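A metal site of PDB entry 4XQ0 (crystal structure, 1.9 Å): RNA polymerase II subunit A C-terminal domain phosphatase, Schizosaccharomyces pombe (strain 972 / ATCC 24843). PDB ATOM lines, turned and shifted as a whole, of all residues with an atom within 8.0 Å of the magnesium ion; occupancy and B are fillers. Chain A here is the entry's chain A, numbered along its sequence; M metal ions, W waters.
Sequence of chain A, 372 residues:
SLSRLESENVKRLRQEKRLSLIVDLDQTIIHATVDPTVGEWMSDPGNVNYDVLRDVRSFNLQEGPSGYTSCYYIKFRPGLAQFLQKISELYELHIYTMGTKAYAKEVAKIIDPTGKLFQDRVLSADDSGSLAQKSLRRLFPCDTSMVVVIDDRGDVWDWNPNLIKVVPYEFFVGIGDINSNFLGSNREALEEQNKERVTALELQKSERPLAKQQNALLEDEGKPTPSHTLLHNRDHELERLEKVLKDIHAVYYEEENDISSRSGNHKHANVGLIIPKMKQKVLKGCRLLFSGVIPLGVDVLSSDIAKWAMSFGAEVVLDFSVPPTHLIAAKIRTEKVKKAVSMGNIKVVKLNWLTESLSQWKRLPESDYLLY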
ATOM      1  N   VAL A  23     -26.503  27.921   0.490  1.00  0.00           N
ATOM      2  CA  VAL A  23     -26.417  26.474   0.294  1.00  0.00           C
ATOM      3  C   VAL A  23     -25.369  25.877   1.237  1.00  0.00           C
ATOM      4  O   VAL A  23     -24.182  26.206   1.177  1.00  0.00           O
ATOM      5  CB  VAL A  23     -26.053  26.115  -1.196  1.00  0.00           C
ATOM      6  CG1 VAL A  23     -25.990  24.607  -1.389  1.00  0.00           C
ATOM      7  CG2 VAL A  23     -27.068  26.724  -2.175  1.00  0.00           C
ATOM      8  N   BFD A  24     -25.835  25.046   2.173  1.00  0.00           N
ATOM      9  CA  BFD A  24     -24.945  24.265   3.017  1.00  0.00           C
ATOM     10  C   BFD A  24     -24.261  23.187   2.162  1.00  0.00           C
ATOM     11  O   BFD A  24     -24.830  22.739   1.153  1.00  0.00           O
ATOM     12  CB  BFD A  24     -25.749  23.616   4.128  1.00  0.00           C
ATOM     13  CG  BFD A  24     -24.842  22.743   5.007  1.00  0.00           C
ATOM     14  OD1 BFD A  24     -23.685  23.268   5.549  1.00  0.00           O
ATOM     15  OD2 BFD A  24     -25.248  21.439   5.277  1.00  0.00           O
ATOM     16 BE   BFD A  24     -22.606  22.557   6.195  1.00  0.00          BE
ATOM     17  F1  BFD A  24     -22.203  23.424   7.248  1.00  0.00           F
ATOM     18  F2  BFD A  24     -22.967  21.250   6.679  1.00  0.00           F
ATOM     19  F3  BFD A  24     -21.557  22.437   5.245  1.00  0.00           F
ATOM     20  N   LEU A  25     -23.080  22.728   2.569  1.00  0.00           N
ATOM     21  CA  LEU A  25     -22.423  21.630   1.868  1.00  0.00           C
ATOM     22  C   LEU A  25     -22.727  20.272   2.509  1.00  0.00           C
ATOM     23  O   LEU A  25     -23.497  19.490   1.948  1.00  0.00           O
ATOM     24  CB  LEU A  25     -20.924  21.852   1.845  1.00  0.00           C
ATOM     25  CG  LEU A  25     -20.415  23.052   1.022  1.00  0.00           C
ATOM     26  CD1 LEU A  25     -18.908  23.112   1.088  1.00  0.00           C
ATOM     27  CD2 LEU A  25     -20.887  22.922  -0.417  1.00  0.00           C
ATOM     28  N   ASP A  26     -22.155  20.023   3.673  1.00  0.00           N
ATOM     29  CA  ASP A  26     -22.146  18.700   4.286  1.00  0.00           C
ATOM     30  C   ASP A  26     -23.546  18.225   4.650  1.00  0.00           C
ATOM     31  O   ASP A  26     -24.285  18.843   5.415  1.00  0.00           O
ATOM     32  CB  ASP A  26     -21.214  18.706   5.497  1.00  0.00           C
ATOM     33  CG  ASP A  26     -19.744  18.882   5.106  1.00  0.00           C
ATOM     34  OD1 ASP A  26     -19.258  18.106   4.248  1.00  0.00           O
ATOM     35  OD2 ASP A  26     -19.089  19.838   5.608  1.00  0.00           O
ATOM     36  N   GLN A  27     -23.900  17.119   4.008  1.00  0.00           N
ATOM     37  CA  GLN A  27     -25.154  16.398   4.165  1.00  0.00           C
ATOM     38  C   GLN A  27     -26.356  17.170   3.628  1.00  0.00           C
ATOM     39  O   GLN A  27     -27.497  16.793   3.857  1.00  0.00           O
ATOM     40  CB  GLN A  27     -25.343  15.989   5.644  1.00  0.00           C
ATOM     41  CG  GLN A  27     -24.245  14.999   6.081  1.00  0.00           C
ATOM     42  CD  GLN A  27     -24.675  14.079   7.222  1.00  0.00           C
ATOM     43  OE1 GLN A  27     -24.605  14.465   8.388  1.00  0.00           O
ATOM     44  NE2 GLN A  27     -25.105  12.866   6.879  1.00  0.00           N
ATOM     45  N   THR A  28     -26.070  18.225   2.864  1.00  0.00           N
ATOM     46  CA  THR A  28     -27.095  18.943   2.103  1.00  0.00           C
ATOM     47  C   THR A  28     -26.943  18.654   0.621  1.00  0.00           C
ATOM     48  O   THR A  28     -27.844  18.098   0.004  1.00  0.00           O
ATOM     49  CB  THR A  28     -27.018  20.456   2.386  1.00  0.00           C
ATOM     50  OG1 THR A  28     -27.389  20.671   3.751  1.00  0.00           O
ATOM     51  CG2 THR A  28     -27.952  21.265   1.464  1.00  0.00           C
ATOM     52  N   ILE A  29     -25.805  19.024   0.022  1.00  0.00           N
ATOM     53  CA  ILE A  29     -25.566  18.662  -1.367  1.00  0.00           C
ATOM     54  C   ILE A  29     -24.398  17.692  -1.571  1.00  0.00           C
ATOM     55  O   ILE A  29     -24.199  17.226  -2.701  1.00  0.00           O
ATOM     56  CB  ILE A  29     -25.320  19.925  -2.257  1.00  0.00           C
ATOM     57  CG1 ILE A  29     -24.129  20.735  -1.765  1.00  0.00           C
ATOM     58  CG2 ILE A  29     -26.570  20.769  -2.319  1.00  0.00           C
ATOM     59  CD1 ILE A  29     -23.605  21.615  -2.807  1.00  0.00           C
ATOM     60  N   ILE A  30     -23.643  17.397  -0.527  1.00  0.00           N
ATOM     61  CA  ILE A  30     -22.599  16.372  -0.588  1.00  0.00           C
ATOM     62  C   ILE A  30     -22.603  15.496   0.670  1.00  0.00           C
ATOM     63  O   ILE A  30     -23.178  15.839   1.682  1.00  0.00           O
ATOM     64  CB  ILE A  30     -21.170  16.979  -0.743  1.00  0.00           C
ATOM     65  CG1 ILE A  30     -20.764  17.758   0.524  1.00  0.00           C
ATOM     66  CG2 ILE A  30     -21.084  17.792  -2.025  1.00  0.00           C
ATOM     67  CD1 ILE A  30     -19.364  18.298   0.501  1.00  0.00           C
ATOM     68  N   TYR A  96     -22.294  28.318   2.383  1.00  0.00           N
ATOM     69  CA  TYR A  96     -22.044  28.651   3.781  1.00  0.00           C
ATOM     70  C   TYR A  96     -21.871  27.338   4.532  1.00  0.00           C
ATOM     71  O   TYR A  96     -22.844  26.634   4.783  1.00  0.00           O
ATOM     72  CB  TYR A  96     -23.209  29.479   4.340  1.00  0.00           C
ATOM     73  CG  TYR A  96     -23.014  30.225   5.620  1.00  0.00           C
ATOM     74  CD1 TYR A  96     -22.096  29.839   6.588  1.00  0.00           C
ATOM     75  CD2 TYR A  96     -23.831  31.324   5.899  1.00  0.00           C
ATOM     76  CE1 TYR A  96     -21.970  30.584   7.774  1.00  0.00           C
ATOM     77  CE2 TYR A  96     -23.718  32.030   7.066  1.00  0.00           C
ATOM     78  CZ  TYR A  96     -22.798  31.657   8.006  1.00  0.00           C
ATOM     79  OH  TYR A  96     -22.709  32.396   9.165  1.00  0.00           O
ATOM     80  N   THR A  97     -20.627  27.024   4.868  1.00  0.00           N
ATOM     81  CA  THR A  97     -20.289  25.745   5.491  1.00  0.00           C
ATOM     82  C   THR A  97     -19.545  25.939   6.802  1.00  0.00           C
ATOM     83  O   THR A  97     -18.928  26.977   7.041  1.00  0.00           O
ATOM     84  CB  THR A  97     -19.422  24.861   4.530  1.00  0.00           C
ATOM     85  OG1 THR A  97     -19.153  23.590   5.131  1.00  0.00           O
ATOM     86  CG2 THR A  97     -18.122  25.533   4.209  1.00  0.00           C
ATOM     87  N   MET A  98     -19.623  24.924   7.656  1.00  0.00           N
ATOM     88  CA  MET A  98     -18.851  24.894   8.883  1.00  0.00           C
ATOM     89  C   MET A  98     -17.492  24.237   8.631  1.00  0.00           C
ATOM     90  O   MET A  98     -16.657  24.190   9.533  1.00  0.00           O
ATOM     91  CB  MET A  98     -19.623  24.154   9.986  1.00  0.00           C
ATOM     92  CG  MET A  98     -20.682  25.010  10.643  1.00  0.00           C
ATOM     93  SD  MET A  98     -19.978  26.425  11.523  1.00  0.00           S
ATOM     94  CE  MET A  98     -21.497  27.176  12.064  1.00  0.00           C
ATOM     95  N   LYS A 134     -24.808  29.714  12.324  1.00  0.00           N
ATOM     96  CA  LYS A 134     -24.747  30.490  11.111  1.00  0.00           C
ATOM     97  C   LYS A 134     -25.718  31.653  11.265  1.00  0.00           C
ATOM     98  O   LYS A 134     -26.616  31.579  12.089  1.00  0.00           O
ATOM     99  CB  LYS A 134     -25.088  29.621   9.895  1.00  0.00           C
ATOM    100  CG  LYS A 134     -24.223  28.384   9.764  1.00  0.00           C
ATOM    101  CD  LYS A 134     -24.610  27.581   8.532  1.00  0.00           C
ATOM    102  CE  LYS A 134     -23.697  26.343   8.349  1.00  0.00           C
ATOM    103  NZ  LYS A 134     -24.119  25.541   7.148  1.00  0.00           N
ATOM    104  N   ILE A 150     -30.918  26.607   2.364  1.00  0.00           N
ATOM    105  CA  ILE A 150     -31.088  25.161   2.428  1.00  0.00           C
ATOM    106  C   ILE A 150     -29.950  24.539   3.243  1.00  0.00           C
ATOM    107  O   ILE A 150     -28.770  24.739   2.955  1.00  0.00           O
ATOM    108  CB  ILE A 150     -31.169  24.510   1.035  1.00  0.00           C
ATOM    109  CG1 ILE A 150     -29.980  24.863   0.132  1.00  0.00           C
ATOM    110  CG2 ILE A 150     -32.461  24.881   0.389  1.00  0.00           C
ATOM    111  CD1 ILE A 150     -29.982  24.101  -1.209  1.00  0.00           C
ATOM    112  N   ASP A 151     -30.344  23.781   4.264  1.00  0.00           N
ATOM    113  CA  ASP A 151     -29.403  23.213   5.224  1.00  0.00           C
ATOM    114  C   ASP A 151     -30.028  21.984   5.871  1.00  0.00           C
ATOM    115  O   ASP A 151     -31.238  21.950   6.081  1.00  0.00           O
ATOM    116  CB  ASP A 151     -29.025  24.288   6.275  1.00  0.00           C
ATOM    117  CG  ASP A 151     -27.705  24.018   7.004  1.00  0.00           C
ATOM    118  OD1 ASP A 151     -27.531  22.907   7.562  1.00  0.00           O
ATOM    119  OD2 ASP A 151     -26.845  24.934   7.046  1.00  0.00           O
ATOM    120  N   ASP A 152     -29.224  20.970   6.175  1.00  0.00           N
ATOM    121  CA  ASP A 152     -29.741  19.777   6.813  1.00  0.00           C
ATOM    122  C   ASP A 152     -29.956  19.978   8.316  1.00  0.00           C
ATOM    123  O   ASP A 152     -30.577  19.142   8.961  1.00  0.00           O
ATOM    124  CB  ASP A 152     -28.810  18.576   6.605  1.00  0.00           C
ATOM    125  CG  ASP A 152     -27.408  18.806   7.178  1.00  0.00           C
ATOM    126  OD1 ASP A 152     -26.664  19.706   6.705  1.00  0.00           O
ATOM    127  OD2 ASP A 152     -27.015  18.041   8.084  1.00  0.00           O
ATOM    128  N   ARG A 153     -29.381  21.043   8.864  1.00  0.00           N
ATOM    129  CA  ARG A 153     -29.517  21.337  10.294  1.00  0.00           C
ATOM    130  C   ARG A 153     -30.326  22.593  10.527  1.00  0.00           C
ATOM    131  O   ARG A 153     -30.016  23.643   9.973  1.00  0.00           O
ATOM    132  CB  ARG A 153     -28.134  21.490  10.930  1.00  0.00           C
ATOM    133  CG  ARG A 153     -27.341  20.212  10.930  1.00  0.00           C
ATOM    134  CD  ARG A 153     -25.997  20.420  11.578  1.00  0.00           C
ATOM    135  NE  ARG A 153     -26.102  20.721  13.003  1.00  0.00           N
ATOM    136  CZ  ARG A 153     -26.038  19.831  13.981  1.00  0.00           C
ATOM    137  NH1 ARG A 153     -25.881  18.539  13.720  1.00  0.00           N
ATOM    138  NH2 ARG A 153     -26.133  20.223  15.239  1.00  0.00           N
ATOM    139  N   VAL A 156     -28.375  24.999  13.766  1.00  0.00           N
ATOM    140  CA  VAL A 156     -27.323  25.995  13.493  1.00  0.00           C
ATOM    141  C   VAL A 156     -27.898  27.324  13.010  1.00  0.00           C
ATOM    142  O   VAL A 156     -27.208  28.336  13.020  1.00  0.00           O
ATOM    143  CB  VAL A 156     -26.270  25.522  12.441  1.00  0.00           C
ATOM    144  CG1 VAL A 156     -25.526  24.371  12.943  1.00  0.00           C
ATOM    145  CG2 VAL A 156     -26.905  25.222  11.088  1.00  0.00           C
ATOM    146  N   TRP A 157     -29.152  27.310  12.583  1.00  0.00           N
ATOM    147  CA  TRP A 157     -29.818  28.500  12.072  1.00  0.00           C
ATOM    148  C   TRP A 157     -30.860  29.023  13.071  1.00  0.00           C
ATOM    149  O   TRP A 157     -31.619  29.925  12.761  1.00  0.00           O
ATOM    150  CB  TRP A 157     -30.476  28.199  10.739  1.00  0.00           C
ATOM    151  CG  TRP A 157     -29.535  28.083   9.595  1.00  0.00           C
ATOM    152  CD1 TRP A 157     -29.087  26.923   8.994  1.00  0.00           C
ATOM    153  CD2 TRP A 157     -28.876  29.156   8.909  1.00  0.00           C
ATOM    154  NE1 TRP A 157     -28.213  27.227   7.979  1.00  0.00           N
ATOM    155  CE2 TRP A 157     -28.071  28.584   7.904  1.00  0.00           C
ATOM    156  CE3 TRP A 157     -28.898  30.554   9.042  1.00  0.00           C
ATOM    157  CZ2 TRP A 157     -27.301  29.349   7.035  1.00  0.00           C
ATOM    158  CZ3 TRP A 157     -28.137  31.305   8.177  1.00  0.00           C
ATOM    159  CH2 TRP A 157     -27.342  30.709   7.193  1.00  0.00           C
ATOM    160  N   VAL A 166     -33.388  20.414   4.954  1.00  0.00           N
ATOM    161  CA  VAL A 166     -33.411  19.284   4.035  1.00  0.00           C
ATOM    162  C   VAL A 166     -33.121  17.991   4.814  1.00  0.00           C
ATOM    163  O   VAL A 166     -32.562  18.004   5.914  1.00  0.00           O
ATOM    164  CB  VAL A 166     -32.402  19.469   2.872  1.00  0.00           C
ATOM    165  CG1 VAL A 166     -32.637  20.830   2.162  1.00  0.00           C
ATOM    166  CG2 VAL A 166     -30.991  19.386   3.353  1.00  0.00           C
ATOM    167  N   PRO A 168     -30.962  15.078   5.828  1.00  0.00           N
ATOM    168  CA  PRO A 168     -29.508  14.913   5.806  1.00  0.00           C
ATOM    169  C   PRO A 168     -29.100  13.808   4.830  1.00  0.00           C
ATOM    170  O   PRO A 168     -29.696  12.740   4.856  1.00  0.00           O
ATOM    171  CB  PRO A 168     -29.159  14.538   7.250  1.00  0.00           C
ATOM    172  CG  PRO A 168     -30.297  15.116   8.069  1.00  0.00           C
ATOM    173  CD  PRO A 168     -31.512  14.930   7.185  1.00  0.00           C
ATOM    174  N   TYR A 169     -28.162  14.120   3.945  1.00  0.00           N
ATOM    175  CA  TYR A 169     -27.726  13.157   2.938  1.00  0.00           C
ATOM    176  C   TYR A 169     -26.736  12.179   3.573  1.00  0.00           C
ATOM    177  O   TYR A 169     -25.663  12.574   4.025  1.00  0.00           O
ATOM    178  CB  TYR A 169     -27.102  13.886   1.731  1.00  0.00           C
ATOM    179  CG  TYR A 169     -26.712  12.968   0.564  1.00  0.00           C
ATOM    180  CD1 TYR A 169     -27.549  11.934   0.135  1.00  0.00           C
ATOM    181  CD2 TYR A 169     -25.523  13.179  -0.129  1.00  0.00           C
ATOM    182  CE1 TYR A 169     -27.183  11.110  -0.933  1.00  0.00           C
ATOM    183  CE2 TYR A 169     -25.157  12.355  -1.197  1.00  0.00           C
ATOM    184  CZ  TYR A 169     -26.000  11.340  -1.596  1.00  0.00           C
ATOM    185  OH  TYR A 169     -25.620  10.541  -2.639  1.00  0.00           O
ATOM    186  N   ASP A 177     -21.447  13.691   9.826  1.00  0.00           N
ATOM    187  CA  ASP A 177     -20.934  14.959   9.313  1.00  0.00           C
ATOM    188  C   ASP A 177     -19.513  15.136   9.863  1.00  0.00           C
ATOM    189  O   ASP A 177     -19.332  15.423  11.045  1.00  0.00           O
ATOM    190  CB  ASP A 177     -21.876  16.102   9.737  1.00  0.00           C
ATOM    191  CG  ASP A 177     -21.389  17.479   9.318  1.00  0.00           C
ATOM    192  OD1 ASP A 177     -20.281  17.584   8.724  1.00  0.00           O
ATOM    193  OD2 ASP A 177     -22.113  18.458   9.624  1.00  0.00           O
ATOM    194  N   ASN A 179     -17.517  17.470   9.528  1.00  0.00           N
ATOM    195  CA  ASN A 179     -17.223  18.871   9.895  1.00  0.00           C
ATOM    196  C   ASN A 179     -18.141  19.398  11.027  1.00  0.00           C
ATOM    197  O   ASN A 179     -18.303  20.596  11.177  1.00  0.00           O
ATOM    198  CB  ASN A 179     -17.348  19.778   8.665  1.00  0.00           C
ATOM    199  CG  ASN A 179     -16.247  19.541   7.652  1.00  0.00           C
ATOM    200  OD1 ASN A 179     -15.089  19.308   8.021  1.00  0.00           O
ATOM    201  ND2 ASN A 179     -16.588  19.579   6.381  1.00  0.00           N
ATOM    202  N   SER A 180     -18.732  18.503  11.813  1.00  0.00           N
ATOM    203  CA  SER A 180     -19.679  18.939  12.866  1.00  0.00           C
ATOM    204  C   SER A 180     -19.024  19.056  14.233  1.00  0.00           C
ATOM    205  O   SER A 180     -19.657  19.513  15.195  1.00  0.00           O
ATOM    206  CB  SER A 180     -20.867  17.984  12.971  1.00  0.00           C
ATOM    207  OG  SER A 180     -20.465  16.713  13.481  1.00  0.00           O
ATOM    208  N   LEU A 183     -19.903  22.161  16.709  1.00  0.00           N
ATOM    209  CA  LEU A 183     -21.217  22.797  16.711  1.00  0.00           C
ATOM    210  C   LEU A 183     -21.791  22.954  18.122  1.00  0.00           C
ATOM    211  O   LEU A 183     -21.799  22.014  18.916  1.00  0.00           O
ATOM    212  CB  LEU A 183     -22.210  21.989  15.856  1.00  0.00           C
ATOM    213  CG  LEU A 183     -21.899  21.822  14.365  1.00  0.00           C
ATOM    214  CD1 LEU A 183     -23.105  21.201  13.652  1.00  0.00           C
ATOM    215  CD2 LEU A 183     -21.506  23.135  13.710  1.00  0.00           C
HETATM  216 MG    MG M   1     -24.653  20.319   6.761  1.00  0.00          MG
HETATM  217  O   HOH W   1     -24.359  19.066   8.270  1.00  0.00           O
HETATM  218  O   HOH W   2     -25.298  21.725   8.198  1.00  0.00           O
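OD2 of BFD 24 sits close to the side-chain hydroxyl (OG1) of Thr 28 (2.7 Å). OD1 of BFD 24 lies within salt-bridge range of the side-chain amino group (NZ) of Lys 134 (2.8 Å). N of BFD 24 is in hydrogen-bond range of O of Ile 150 (3.1 Å). The side-chain amide nitrogen of Asn 179 sits at hydrogen-bond distance from the side-chain carboxylate of Asp 26, 2.6 Å away. The side-chain carboxylate (OD1) of Asp 151 is in hydrogen-bond range of the backbone NH (N) of Arg 153 (2.9 Å). NZ of Lys 134 is in salt-bridge range of OD2 of Asp 151 (2.8 Å). The backbone NH (N) of Val 166 lies within hydrogen-bond range of the backbone carbonyl oxygen (O) of Asp 151 (2.9 Å). The side-chain carboxylate of Asp 151 lies within hydrogen-bond range of the indole nitrogen of Trp 157 (2.8 Å).
Merely in contact with the magnesium ion: Asp 151. The nearest printed residue that does not touch the magnesium ion is Thr 28 (4.1 Å).
F2 of BFD 24 binds the magnesium ion (1.9 Å). OD2 of BFD 24 is bound to the magnesium ion, at 2.0 Å. Water W1 is bound to the magnesium ion (2.0 Å). The magnesium ion is bound by O of Asp 26 (2.0 Å). OD1 of Asp 152 binds the magnesium ion (2.1 Å). The magnesium ion is bound by water W2.
Water W2 lies within hydrogen-bond range of the side-chain carboxylate of Asp 151 and OD1 of BFD 24. Water W1 bridges the side-chain carboxylate (OD2) of Asp 177 (2.7 Å) and the side-chain carboxylate (OD2) of Asp 152 (2.9 Å).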
